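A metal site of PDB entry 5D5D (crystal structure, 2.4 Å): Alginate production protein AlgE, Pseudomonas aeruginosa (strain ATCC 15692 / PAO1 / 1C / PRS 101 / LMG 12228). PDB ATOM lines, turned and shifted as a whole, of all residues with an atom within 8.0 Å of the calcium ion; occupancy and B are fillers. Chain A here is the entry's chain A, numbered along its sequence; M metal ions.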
ATOM      1  N   ASN A  54      12.983  -8.358  12.393  1.00  0.00           N
ATOM      2  CA  ASN A  54      13.056  -7.430  11.290  1.00  0.00           C
ATOM      3  C   ASN A  54      12.633  -6.050  11.777  1.00  0.00           C
ATOM      4  O   ASN A  54      11.450  -5.828  11.983  1.00  0.00           O
ATOM      5  CB  ASN A  54      12.180  -7.929  10.111  1.00  0.00           C
ATOM      6  CG  ASN A  54      11.907  -6.983   8.951  1.00  0.00           C
ATOM      7  OD1 ASN A  54      12.505  -5.925   8.778  1.00  0.00           O
ATOM      8  ND2 ASN A  54      10.959  -7.371   8.132  1.00  0.00           N
ATOM      9  N   ASP A  55      13.556  -5.107  11.897  1.00  0.00           N
ATOM     10  CA  ASP A  55      14.985  -5.241  11.680  1.00  0.00           C
ATOM     11  C   ASP A  55      15.647  -4.620  12.888  1.00  0.00           C
ATOM     12  O   ASP A  55      15.382  -3.459  13.221  1.00  0.00           O
ATOM     13  CB  ASP A  55      15.414  -4.501  10.370  1.00  0.00           C
ATOM     14  CG  ASP A  55      16.887  -4.577  10.001  1.00  0.00           C
ATOM     15  OD1 ASP A  55      17.725  -4.852  10.887  1.00  0.00           O
ATOM     16  OD2 ASP A  55      17.203  -4.373   8.837  1.00  0.00           O
ATOM     17  N   ARG A  56      16.527  -5.398  13.527  1.00  0.00           N
ATOM     18  CA  ARG A  56      17.281  -5.057  14.742  1.00  0.00           C
ATOM     19  C   ARG A  56      18.012  -3.691  14.662  1.00  0.00           C
ATOM     20  O   ARG A  56      18.217  -3.064  15.691  1.00  0.00           O
ATOM     21  CB  ARG A  56      18.290  -6.166  14.976  1.00  0.00           C
ATOM     22  CG  ARG A  56      18.592  -6.483  16.400  1.00  0.00           C
ATOM     23  CD  ARG A  56      19.404  -7.740  16.438  1.00  0.00           C
ATOM     24  NE  ARG A  56      20.600  -7.571  15.633  1.00  0.00           N
ATOM     25  CZ  ARG A  56      21.070  -8.446  14.762  1.00  0.00           C
ATOM     26  NH1 ARG A  56      22.175  -8.189  14.072  1.00  0.00           N
ATOM     27  NH2 ARG A  56      20.445  -9.605  14.569  1.00  0.00           N
ATOM     28  N   ASP A  57      18.452  -3.266  13.459  1.00  0.00           N
ATOM     29  CA  ASP A  57      19.131  -1.985  13.277  1.00  0.00           C
ATOM     30  C   ASP A  57      18.197  -0.956  12.650  1.00  0.00           C
ATOM     31  O   ASP A  57      18.641   0.114  12.220  1.00  0.00           O
ATOM     32  CB  ASP A  57      20.428  -2.124  12.468  1.00  0.00           C
ATOM     33  CG  ASP A  57      20.217  -2.777  11.121  1.00  0.00           C
ATOM     34  OD1 ASP A  57      19.594  -2.133  10.229  1.00  0.00           O
ATOM     35  OD2 ASP A  57      20.642  -3.955  10.964  1.00  0.00           O
ATOM     36  N   LEU A  58      16.899  -1.284  12.584  1.00  0.00           N
ATOM     37  CA  LEU A  58      15.817  -0.460  12.029  1.00  0.00           C
ATOM     38  C   LEU A  58      16.070  -0.090  10.560  1.00  0.00           C
ATOM     39  O   LEU A  58      15.764   1.013  10.139  1.00  0.00           O
ATOM     40  CB  LEU A  58      15.589   0.810  12.914  1.00  0.00           C
ATOM     41  CG  LEU A  58      15.534   0.607  14.430  1.00  0.00           C
ATOM     42  CD1 LEU A  58      15.482   1.909  15.115  1.00  0.00           C
ATOM     43  CD2 LEU A  58      14.346  -0.250  14.838  1.00  0.00           C
ATOM     44  N   GLY A  59      16.663  -1.033   9.822  1.00  0.00           N
ATOM     45  CA  GLY A  59      17.012  -0.867   8.411  1.00  0.00           C
ATOM     46  C   GLY A  59      18.055   0.180   8.095  1.00  0.00           C
ATOM     47  O   GLY A  59      17.961   0.855   7.060  1.00  0.00           O
ATOM     48  N   THR A  60      19.071   0.345   8.981  1.00  0.00           N
ATOM     49  CA  THR A  60      20.107   1.356   8.826  1.00  0.00           C
ATOM     50  C   THR A  60      21.508   0.731   8.676  1.00  0.00           C
ATOM     51  O   THR A  60      22.494   1.462   8.678  1.00  0.00           O
ATOM     52  CB  THR A  60      20.104   2.356  10.032  1.00  0.00           C
ATOM     53  OG1 THR A  60      20.589   1.710  11.223  1.00  0.00           O
ATOM     54  CG2 THR A  60      18.760   2.984  10.290  1.00  0.00           C
ATOM     55  N   ALA A  61      21.593  -0.603   8.629  1.00  0.00           N
ATOM     56  CA  ALA A  61      22.848  -1.347   8.551  1.00  0.00           C
ATOM     57  C   ALA A  61      22.625  -2.698   7.951  1.00  0.00           C
ATOM     58  O   ALA A  61      21.622  -3.314   8.293  1.00  0.00           O
ATOM     59  CB  ALA A  61      23.426  -1.531   9.958  1.00  0.00           C
ATOM     60  N   PRO A  62      23.544  -3.244   7.123  1.00  0.00           N
ATOM     61  CA  PRO A  62      23.355  -4.633   6.642  1.00  0.00           C
ATOM     62  C   PRO A  62      23.254  -5.574   7.842  1.00  0.00           C
ATOM     63  O   PRO A  62      23.995  -5.409   8.803  1.00  0.00           O
ATOM     64  CB  PRO A  62      24.621  -4.934   5.820  1.00  0.00           C
ATOM     65  CG  PRO A  62      25.549  -3.792   6.054  1.00  0.00           C
ATOM     66  CD  PRO A  62      24.795  -2.638   6.600  1.00  0.00           C
ATOM     67  N   GLY A  63      22.284  -6.489   7.789  1.00  0.00           N
ATOM     68  CA  GLY A  63      21.998  -7.448   8.840  1.00  0.00           C
ATOM     69  C   GLY A  63      20.794  -7.036   9.666  1.00  0.00           C
ATOM     70  O   GLY A  63      20.033  -6.143   9.259  1.00  0.00           O
ATOM     71  N   GLY A  64      20.620  -7.677  10.814  1.00  0.00           N
ATOM     72  CA  GLY A  64      19.536  -7.348  11.721  1.00  0.00           C
ATOM     73  C   GLY A  64      18.213  -8.035  11.441  1.00  0.00           C
ATOM     74  O   GLY A  64      17.213  -7.721  12.083  1.00  0.00           O
ATOM     75  N   THR A  65      18.219  -8.987  10.484  1.00  0.00           N
ATOM     76  CA  THR A  65      17.027  -9.741  10.113  1.00  0.00           C
ATOM     77  C   THR A  65      17.166 -11.242  10.472  1.00  0.00           C
ATOM     78  O   THR A  65      18.274 -11.768  10.582  1.00  0.00           O
ATOM     79  CB  THR A  65      16.621  -9.505   8.638  1.00  0.00           C
ATOM     80  OG1 THR A  65      17.674  -9.949   7.787  1.00  0.00           O
ATOM     81  CG2 THR A  65      16.286  -8.060   8.344  1.00  0.00           C
ATOM     82  N   ASP A 295      26.318  -6.388  10.466  1.00  0.00           N
ATOM     83  CA  ASP A 295      25.795  -7.413  11.386  1.00  0.00           C
ATOM     84  C   ASP A 295      26.772  -7.832  12.531  1.00  0.00           C
ATOM     85  O   ASP A 295      26.479  -8.773  13.291  1.00  0.00           O
ATOM     86  CB  ASP A 295      25.289  -8.661  10.621  1.00  0.00           C
ATOM     87  CG  ASP A 295      24.064  -9.320  11.249  1.00  0.00           C
ATOM     88  OD1 ASP A 295      24.028 -10.561  11.316  1.00  0.00           O
ATOM     89  OD2 ASP A 295      23.124  -8.599  11.617  1.00  0.00           O
ATOM     90  N   ASN A 416      20.062  -2.327  17.906  1.00  0.00           N
ATOM     91  CA  ASN A 416      21.473  -1.897  17.881  1.00  0.00           C
ATOM     92  C   ASN A 416      21.709  -0.652  16.989  1.00  0.00           C
ATOM     93  O   ASN A 416      22.845  -0.204  16.832  1.00  0.00           O
ATOM     94  CB  ASN A 416      22.391  -3.051  17.498  1.00  0.00           C
ATOM     95  CG  ASN A 416      22.108  -3.681  16.171  1.00  0.00           C
ATOM     96  OD1 ASN A 416      21.659  -3.037  15.233  1.00  0.00           O
ATOM     97  ND2 ASN A 416      22.397  -4.957  16.066  1.00  0.00           N
ATOM     98  N   ASP A 476      13.209   2.038   9.326  1.00  0.00           N
ATOM     99  CA  ASP A 476      11.931   1.370   9.034  1.00  0.00           C
ATOM    100  C   ASP A 476      10.857   1.948   9.995  1.00  0.00           C
ATOM    101  O   ASP A 476      11.191   2.350  11.118  1.00  0.00           O
ATOM    102  CB  ASP A 476      12.052  -0.150   9.192  1.00  0.00           C
ATOM    103  CG  ASP A 476      13.222  -0.797   8.469  1.00  0.00           C
ATOM    104  OD1 ASP A 476      13.728  -0.204   7.483  1.00  0.00           O
ATOM    105  OD2 ASP A 476      13.610  -1.925   8.846  1.00  0.00           O
HETATM  106 CA    CA M   1      19.463  -4.132   8.757  1.00  0.00          CA
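The calcium ion is bound by O of Gly 63 (2.1 Å), OD2 of Asp 55 (2.3 Å), O of Ala 61 (2.4 Å), OD1 of Asp 57 (2.5 Å), OD2 of Asp 57 (2.5 Å) and OD1 of Asp 55 (2.8 Å).
N of Gly 59 lies close to OD1 of Asp 57 (3.2 Å). O of Asp 57 is in hydrogen-bond range of OG1 of Thr 60.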
